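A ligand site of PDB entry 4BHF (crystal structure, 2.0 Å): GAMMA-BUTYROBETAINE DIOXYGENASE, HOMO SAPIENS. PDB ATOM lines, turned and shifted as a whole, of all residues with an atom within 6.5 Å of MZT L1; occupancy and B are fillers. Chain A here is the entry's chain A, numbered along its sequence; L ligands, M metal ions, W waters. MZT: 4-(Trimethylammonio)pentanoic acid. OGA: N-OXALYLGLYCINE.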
ATOM      1  N   THR A 175       6.595   5.607  11.983  1.00  0.00           N
ATOM      2  CA  THR A 175       5.832   4.371  11.749  1.00  0.00           C
ATOM      3  C   THR A 175       6.319   3.714  10.432  1.00  0.00           C
ATOM      4  O   THR A 175       7.191   4.252   9.742  1.00  0.00           O
ATOM      5  CB  THR A 175       4.313   4.630  11.670  1.00  0.00           C
ATOM      6  OG1 THR A 175       3.999   5.278  10.432  1.00  0.00           O
ATOM      7  CG2 THR A 175       3.808   5.538  12.817  1.00  0.00           C
ATOM      8  N   TYR A 177       5.062   3.737   7.686  1.00  0.00           N
ATOM      9  CA  TYR A 177       4.754   4.595   6.538  1.00  0.00           C
ATOM     10  C   TYR A 177       5.724   5.759   6.432  1.00  0.00           C
ATOM     11  O   TYR A 177       5.614   6.549   5.499  1.00  0.00           O
ATOM     12  CB  TYR A 177       3.293   5.077   6.545  1.00  0.00           C
ATOM     13  CG  TYR A 177       2.347   3.952   6.208  1.00  0.00           C
ATOM     14  CD1 TYR A 177       2.197   3.525   4.896  1.00  0.00           C
ATOM     15  CD2 TYR A 177       1.665   3.270   7.208  1.00  0.00           C
ATOM     16  CE1 TYR A 177       1.360   2.469   4.578  1.00  0.00           C
ATOM     17  CE2 TYR A 177       0.842   2.210   6.904  1.00  0.00           C
ATOM     18  CZ  TYR A 177       0.697   1.814   5.583  1.00  0.00           C
ATOM     19  OH  TYR A 177      -0.085   0.788   5.279  1.00  0.00           O
ATOM     20  N   TRP A 181       4.675  11.262   5.394  1.00  0.00           N
ATOM     21  CA  TRP A 181       4.164  10.429   4.300  1.00  0.00           C
ATOM     22  C   TRP A 181       3.276  11.217   3.372  1.00  0.00           C
ATOM     23  O   TRP A 181       2.714  12.231   3.781  1.00  0.00           O
ATOM     24  CB  TRP A 181       3.400   9.202   4.824  1.00  0.00           C
ATOM     25  CG  TRP A 181       2.824   9.329   6.180  1.00  0.00           C
ATOM     26  CD1 TRP A 181       3.398   8.963   7.366  1.00  0.00           C
ATOM     27  CD2 TRP A 181       1.520   9.840   6.513  1.00  0.00           C
ATOM     28  NE1 TRP A 181       2.560   9.242   8.396  1.00  0.00           N
ATOM     29  CE2 TRP A 181       1.403   9.795   7.908  1.00  0.00           C
ATOM     30  CE3 TRP A 181       0.439  10.317   5.763  1.00  0.00           C
ATOM     31  CZ2 TRP A 181       0.257  10.205   8.566  1.00  0.00           C
ATOM     32  CZ3 TRP A 181      -0.689  10.727   6.419  1.00  0.00           C
ATOM     33  CH2 TRP A 181      -0.778  10.673   7.812  1.00  0.00           C
ATOM     34  N   VAL A 183       0.011  11.557   1.016  1.00  0.00           N
ATOM     35  CA  VAL A 183      -1.323  11.092   0.660  1.00  0.00           C
ATOM     36  C   VAL A 183      -1.599  11.593  -0.757  1.00  0.00           C
ATOM     37  O   VAL A 183      -1.864  12.778  -0.973  1.00  0.00           O
ATOM     38  CB  VAL A 183      -2.400  11.612   1.611  1.00  0.00           C
ATOM     39  CG1 VAL A 183      -3.742  11.004   1.273  1.00  0.00           C
ATOM     40  CG2 VAL A 183      -2.019  11.331   3.057  1.00  0.00           C
ATOM     41  N   ASN A 190      -0.261   0.579  -1.491  1.00  0.00           N
ATOM     42  CA  ASN A 190      -0.179  -0.248  -0.292  1.00  0.00           C
ATOM     43  C   ASN A 190      -1.248   0.064   0.782  1.00  0.00           C
ATOM     44  O   ASN A 190      -1.277  -0.569   1.823  1.00  0.00           O
ATOM     45  CB  ASN A 190       1.245  -0.217   0.304  1.00  0.00           C
ATOM     46  CG  ASN A 190       1.633   1.128   0.919  1.00  0.00           C
ATOM     47  OD1 ASN A 190       0.816   2.029   1.178  1.00  0.00           O
ATOM     48  ND2 ASN A 190       2.921   1.244   1.192  1.00  0.00           N
ATOM     49  N   ASN A 191      -2.145   1.022   0.503  1.00  0.00           N
ATOM     50  CA  ASN A 191      -3.105   1.514   1.477  1.00  0.00           C
ATOM     51  C   ASN A 191      -4.230   2.261   0.769  1.00  0.00           C
ATOM     52  O   ASN A 191      -3.963   3.054  -0.134  1.00  0.00           O
ATOM     53  CB  ASN A 191      -2.403   2.489   2.426  1.00  0.00           C
ATOM     54  CG  ASN A 191      -3.164   2.693   3.726  1.00  0.00           C
ATOM     55  OD1 ASN A 191      -4.170   3.421   3.768  1.00  0.00           O
ATOM     56  ND2 ASN A 191      -2.685   2.052   4.785  1.00  0.00           N
ATOM     57  N   VAL A 192      -5.472   2.066   1.184  1.00  0.00           N
ATOM     58  CA  VAL A 192      -6.583   2.751   0.513  1.00  0.00           C
ATOM     59  C   VAL A 192      -6.489   4.284   0.620  1.00  0.00           C
ATOM     60  O   VAL A 192      -7.037   5.019  -0.219  1.00  0.00           O
ATOM     61  CB  VAL A 192      -7.944   2.326   1.118  1.00  0.00           C
ATOM     62  CG1 VAL A 192      -8.150   0.840   0.946  1.00  0.00           C
ATOM     63  CG2 VAL A 192      -8.009   2.712   2.587  1.00  0.00           C
ATOM     64  N   ALA A 193      -5.758   4.760   1.621  1.00  0.00           N
ATOM     65  CA  ALA A 193      -5.501   6.200   1.703  1.00  0.00           C
ATOM     66  C   ALA A 193      -4.811   6.711   0.431  1.00  0.00           C
ATOM     67  O   ALA A 193      -5.060   7.814  -0.009  1.00  0.00           O
ATOM     68  CB  ALA A 193      -4.661   6.510   2.927  1.00  0.00           C
ATOM     69  N   TYR A 194      -3.982   5.868  -0.170  1.00  0.00           N
ATOM     70  CA  TYR A 194      -3.172   6.276  -1.334  1.00  0.00           C
ATOM     71  C   TYR A 194      -3.876   5.961  -2.685  1.00  0.00           C
ATOM     72  O   TYR A 194      -3.269   5.503  -3.644  1.00  0.00           O
ATOM     73  CB  TYR A 194      -1.804   5.604  -1.232  1.00  0.00           C
ATOM     74  CG  TYR A 194      -0.984   5.974   0.044  1.00  0.00           C
ATOM     75  CD1 TYR A 194      -1.167   7.190   0.740  1.00  0.00           C
ATOM     76  CD2 TYR A 194       0.013   5.112   0.498  1.00  0.00           C
ATOM     77  CE1 TYR A 194      -0.403   7.493   1.865  1.00  0.00           C
ATOM     78  CE2 TYR A 194       0.780   5.405   1.603  1.00  0.00           C
ATOM     79  CZ  TYR A 194       0.566   6.588   2.290  1.00  0.00           C
ATOM     80  OH  TYR A 194       1.357   6.842   3.373  1.00  0.00           O
ATOM     81  N   HIS A 202     -12.855   7.056  10.114  1.00  0.00           N
ATOM     82  CA  HIS A 202     -11.884   6.156  10.692  1.00  0.00           C
ATOM     83  C   HIS A 202     -10.921   6.933  11.602  1.00  0.00           C
ATOM     84  O   HIS A 202     -10.812   8.163  11.487  1.00  0.00           O
ATOM     85  CB  HIS A 202     -11.082   5.459   9.588  1.00  0.00           C
ATOM     86  CG  HIS A 202     -10.207   6.365   8.775  1.00  0.00           C
ATOM     87  ND1 HIS A 202     -10.711   7.185   7.796  1.00  0.00           N
ATOM     88  CD2 HIS A 202      -8.866   6.567   8.789  1.00  0.00           C
ATOM     89  CE1 HIS A 202      -9.714   7.859   7.230  1.00  0.00           C
ATOM     90  NE2 HIS A 202      -8.587   7.490   7.805  1.00  0.00           N
ATOM     91  N   THR A 203     -10.290   6.198  12.504  1.00  0.00           N
ATOM     92  CA  THR A 203      -9.034   6.617  13.142  1.00  0.00           C
ATOM     93  C   THR A 203      -7.875   5.962  12.379  1.00  0.00           C
ATOM     94  O   THR A 203      -8.069   4.912  11.791  1.00  0.00           O
ATOM     95  CB  THR A 203      -8.969   6.203  14.614  1.00  0.00           C
ATOM     96  OG1 THR A 203      -9.132   4.782  14.773  1.00  0.00           O
ATOM     97  CG2 THR A 203     -10.088   6.881  15.416  1.00  0.00           C
ATOM     98  N   ASP A 204      -6.711   6.608  12.390  1.00  0.00           N
ATOM     99  CA  ASP A 204      -5.490   6.068  11.817  1.00  0.00           C
ATOM    100  C   ASP A 204      -4.804   5.082  12.714  1.00  0.00           C
ATOM    101  O   ASP A 204      -4.713   5.225  13.949  1.00  0.00           O
ATOM    102  CB  ASP A 204      -4.504   7.207  11.465  1.00  0.00           C
ATOM    103  CG  ASP A 204      -4.713   7.756  10.071  1.00  0.00           C
ATOM    104  OD1 ASP A 204      -5.882   7.777   9.634  1.00  0.00           O
ATOM    105  OD2 ASP A 204      -3.707   8.158   9.423  1.00  0.00           O
ATOM    106  N   TYR A 205      -4.408   3.996  12.059  1.00  0.00           N
ATOM    107  CA  TYR A 205      -3.473   3.039  12.553  1.00  0.00           C
ATOM    108  C   TYR A 205      -4.006   2.192  13.727  1.00  0.00           C
ATOM    109  O   TYR A 205      -3.249   1.872  14.632  1.00  0.00           O
ATOM    110  CB  TYR A 205      -2.143   3.712  12.868  1.00  0.00           C
ATOM    111  CG  TYR A 205      -0.925   3.161  12.084  1.00  0.00           C
ATOM    112  CD1 TYR A 205      -0.788   1.801  11.818  1.00  0.00           C
ATOM    113  CD2 TYR A 205       0.077   4.008  11.610  1.00  0.00           C
ATOM    114  CE1 TYR A 205       0.316   1.307  11.129  1.00  0.00           C
ATOM    115  CE2 TYR A 205       1.195   3.523  10.939  1.00  0.00           C
ATOM    116  CZ  TYR A 205       1.299   2.168  10.691  1.00  0.00           C
ATOM    117  OH  TYR A 205       2.390   1.658  10.038  1.00  0.00           O
ATOM    118  N   PRO A 206      -5.290   1.791  13.709  1.00  0.00           N
ATOM    119  CA  PRO A 206      -5.597   0.798  14.767  1.00  0.00           C
ATOM    120  C   PRO A 206      -4.866  -0.539  14.602  1.00  0.00           C
ATOM    121  O   PRO A 206      -4.910  -1.374  15.524  1.00  0.00           O
ATOM    122  CB  PRO A 206      -7.113   0.612  14.654  1.00  0.00           C
ATOM    123  CG  PRO A 206      -7.408   0.891  13.198  1.00  0.00           C
ATOM    124  CD  PRO A 206      -6.438   2.016  12.814  1.00  0.00           C
ATOM    125  N   ALA A 207      -4.171  -0.757  13.485  1.00  0.00           N
ATOM    126  CA  ALA A 207      -3.324  -1.967  13.366  1.00  0.00           C
ATOM    127  C   ALA A 207      -2.167  -1.964  14.367  1.00  0.00           C
ATOM    128  O   ALA A 207      -1.500  -2.983  14.544  1.00  0.00           O
ATOM    129  CB  ALA A 207      -2.822  -2.153  11.947  1.00  0.00           C
ATOM    130  N   GLN A 215      -2.446  13.547  14.898  1.00  0.00           N
ATOM    131  CA  GLN A 215      -2.175  13.465  13.503  1.00  0.00           C
ATOM    132  C   GLN A 215      -2.065  14.869  12.912  1.00  0.00           C
ATOM    133  O   GLN A 215      -2.772  15.765  13.306  1.00  0.00           O
ATOM    134  CB  GLN A 215      -3.287  12.695  12.803  1.00  0.00           C
ATOM    135  CG  GLN A 215      -3.146  12.642  11.299  1.00  0.00           C
ATOM    136  CD  GLN A 215      -4.038  11.596  10.616  1.00  0.00           C
ATOM    137  OE1 GLN A 215      -4.247  11.667   9.404  1.00  0.00           O
ATOM    138  NE2 GLN A 215      -4.560  10.642  11.381  1.00  0.00           N
ATOM    139  N   ASP A 261      -2.297  -5.137   8.861  1.00  0.00           N
ATOM    140  CA  ASP A 261      -1.663  -4.331   7.818  1.00  0.00           C
ATOM    141  C   ASP A 261      -0.401  -5.032   7.380  1.00  0.00           C
ATOM    142  O   ASP A 261       0.493  -5.242   8.193  1.00  0.00           O
ATOM    143  CB  ASP A 261      -1.311  -2.938   8.314  1.00  0.00           C
ATOM    144  CG  ASP A 261      -1.151  -1.926   7.189  1.00  0.00           C
ATOM    145  OD1 ASP A 261      -1.662  -2.134   6.056  1.00  0.00           O
ATOM    146  OD2 ASP A 261      -0.497  -0.877   7.437  1.00  0.00           O
ATOM    147  N   ASN A 292     -10.698   1.597  11.919  1.00  0.00           N
ATOM    148  CA  ASN A 292     -10.524   1.841  10.507  1.00  0.00           C
ATOM    149  C   ASN A 292     -11.117   0.611   9.753  1.00  0.00           C
ATOM    150  O   ASN A 292     -10.715  -0.529   9.984  1.00  0.00           O
ATOM    151  CB  ASN A 292      -9.057   2.079  10.205  1.00  0.00           C
ATOM    152  CG  ASN A 292      -8.814   2.424   8.749  1.00  0.00           C
ATOM    153  OD1 ASN A 292      -9.694   2.191   7.893  1.00  0.00           O
ATOM    154  ND2 ASN A 292      -7.674   2.960   8.453  1.00  0.00           N
ATOM    155  N   ALA A 294     -10.970  -0.162   6.672  1.00  0.00           N
ATOM    156  CA  ALA A 294     -10.088  -0.694   5.646  1.00  0.00           C
ATOM    157  C   ALA A 294      -9.160  -1.723   6.250  1.00  0.00           C
ATOM    158  O   ALA A 294      -8.955  -2.765   5.644  1.00  0.00           O
ATOM    159  CB  ALA A 294      -9.303   0.425   4.942  1.00  0.00           C
ATOM    160  N   THR A 295      -8.654  -1.478   7.469  1.00  0.00           N
ATOM    161  CA  THR A 295      -7.680  -2.358   8.078  1.00  0.00           C
ATOM    162  C   THR A 295      -8.237  -3.350   9.088  1.00  0.00           C
ATOM    163  O   THR A 295      -7.521  -4.212   9.578  1.00  0.00           O
ATOM    164  CB  THR A 295      -6.531  -1.564   8.738  1.00  0.00           C
ATOM    165  OG1 THR A 295      -7.026  -0.837   9.875  1.00  0.00           O
ATOM    166  CG2 THR A 295      -5.952  -0.592   7.716  1.00  0.00           C
ATOM    167  N   HIS A 347     -12.100  10.796  11.112  1.00  0.00           N
ATOM    168  CA  HIS A 347     -12.002  11.663   9.997  1.00  0.00           C
ATOM    169  C   HIS A 347     -12.155  10.847   8.718  1.00  0.00           C
ATOM    170  O   HIS A 347     -12.058   9.603   8.721  1.00  0.00           O
ATOM    171  CB  HIS A 347     -10.659  12.388  10.022  1.00  0.00           C
ATOM    172  CG  HIS A 347      -9.474  11.486   9.870  1.00  0.00           C
ATOM    173  ND1 HIS A 347      -8.984  10.725  10.909  1.00  0.00           N
ATOM    174  CD2 HIS A 347      -8.675  11.248   8.804  1.00  0.00           C
ATOM    175  CE1 HIS A 347      -7.936  10.033  10.489  1.00  0.00           C
ATOM    176  NE2 HIS A 347      -7.725  10.340   9.217  1.00  0.00           N
ATOM    177  N   TYR A 366       2.619  11.875  12.411  1.00  0.00           N
ATOM    178  CA  TYR A 366       2.011  11.574  13.674  1.00  0.00           C
ATOM    179  C   TYR A 366       2.890  12.075  14.826  1.00  0.00           C
ATOM    180  O   TYR A 366       4.092  12.273  14.659  1.00  0.00           O
ATOM    181  CB  TYR A 366       1.844  10.061  13.822  1.00  0.00           C
ATOM    182  CG  TYR A 366       0.940   9.391  12.794  1.00  0.00           C
ATOM    183  CD1 TYR A 366      -0.392   9.758  12.646  1.00  0.00           C
ATOM    184  CD2 TYR A 366       1.425   8.356  12.002  1.00  0.00           C
ATOM    185  CE1 TYR A 366      -1.213   9.128  11.721  1.00  0.00           C
ATOM    186  CE2 TYR A 366       0.617   7.708  11.087  1.00  0.00           C
ATOM    187  CZ  TYR A 366      -0.697   8.088  10.941  1.00  0.00           C
ATOM    188  OH  TYR A 366      -1.502   7.431  10.007  1.00  0.00           O
HETATM  189  N1  MZT L   1      -1.600   6.215   6.325  1.00  0.00           N
HETATM  190  C8  MZT L   1      -0.301   6.651   6.886  1.00  0.00           C
HETATM  191  O4  MZT L   1      -4.118   2.368   7.664  1.00  0.00           O
HETATM  192  C5  MZT L   1      -4.571   3.239   8.430  1.00  0.00           C
HETATM  193  O7  MZT L   1      -4.978   2.899   9.537  1.00  0.00           O
HETATM  194  C6  MZT L   1      -4.700   4.723   8.099  1.00  0.00           C
HETATM  195  C2  MZT L   1      -2.461   5.669   7.437  1.00  0.00           C
HETATM  196  C9  MZT L   1      -2.218   7.409   5.739  1.00  0.00           C
HETATM  197  C10 MZT L   1      -1.358   5.261   5.225  1.00  0.00           C
HETATM  198  C3  MZT L   1      -3.830   5.192   6.941  1.00  0.00           C
HETATM  199  C21 MZT L   1      -1.833   4.545   8.232  1.00  0.00           C
HETATM  200  C1  OGA L   2      -5.454   9.155   5.580  1.00  0.00           C
HETATM  201  C2  OGA L   2      -6.511  10.168   5.551  1.00  0.00           C
HETATM  202  C4  OGA L   2      -7.402  12.154   4.547  1.00  0.00           C
HETATM  203  C5  OGA L   2      -7.467  12.748   3.174  1.00  0.00           C
HETATM  204  O1  OGA L   2      -5.489   8.308   6.489  1.00  0.00           O
HETATM  205  O2  OGA L   2      -4.537   9.207   4.722  1.00  0.00           O
HETATM  206  O2' OGA L   2      -7.413  10.132   6.373  1.00  0.00           O
HETATM  207  O3  OGA L   2      -8.150  13.768   3.109  1.00  0.00           O
HETATM  208  N1  OGA L   2      -6.407  11.108   4.608  1.00  0.00           N
HETATM  209  O4  OGA L   2      -6.913  12.213   2.184  1.00  0.00           O
HETATM  210 ZN    ZN M   1      -6.815   8.725   7.959  1.00  0.00          ZN
HETATM  211  O   HOH W   1      -2.691   0.473   8.972  1.00  0.00           O
HETATM  212  O   HOH W   2      -6.211   2.662   5.580  1.00  0.00           O
HETATM  213  O   HOH W   3      -4.521   0.390  10.748  1.00  0.00           O
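Water W1 bridges O4 of MZT L1 (2.7 Å) and OD2 of Asp 261 (3.0 Å). Water W3 lies within hydrogen-bond range of O7 of MZT L1 (2.8 Å), OG1 of Thr 295 (2.9 Å) and N of Ala 207 (3.0 Å). Water W2 lies within hydrogen-bond range of OD1 of Asn 191, O4 of MZT L1 and ND2 of Asn 292.
Merely in contact with MZT L1: Tyr 177 (3.8 Å), Trp 181 (3.7 Å), Ala 193 (3.8 Å), Tyr 194 (3.6 Å), Asp 204 (3.4 Å), Pro 206 (3.7 Å), Thr 295 (3.5 Å) and Tyr 366 (3.3 Å). Hydrophobic or aromatic side chains that line MZT L1: Tyr 177, Trp 181, Ala 193, Tyr 194, Tyr 205 and Pro 206. 11 residues have an atom within 4 Å of MZT L1: Tyr 177, Trp 181, Asn 191, Ala 193, Tyr 194, Asp 204, Tyr 205, Pro 206, Asn 292, Thr 295 and Tyr 366. The nearest printed residue that does not touch MZT L1 is Thr 203 (4.3 Å).
N of Tyr 205 sits at hydrogen-bond distance from O7 of MZT L1. An oxygen (O7) of MZT L1 lies within hydrogen-bond range of the side-chain amide nitrogen of Asn 292. The side-chain amide nitrogen (ND2) of Asn 191 lies within hydrogen-bond range of an oxygen (O4) of MZT L1 (3.2 Å).
OD2 of Asp 204 lies close to NE2 of Gln 215 (3.3 Å). The side-chain amide nitrogen of Asn 191 is in hydrogen-bond range of the side-chain hydroxyl of Tyr 177. The side-chain amide oxygen (OD1) of Asn 292 is in hydrogen-bond range of the backbone NH (N) of Ala 294 (2.9 Å). The backbone NH (N) of Tyr 177 sits close to the side-chain hydroxyl (OG1) of Thr 175. The side-chain carboxylate of Asp 261 lies within hydrogen-bond range of the side-chain hydroxyl of Tyr 177 (2.8 Å). The side-chain amide oxygen (OD1) of Asn 191 lies within hydrogen-bond range of the backbone NH (N) of Ala 193 (3.0 Å).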
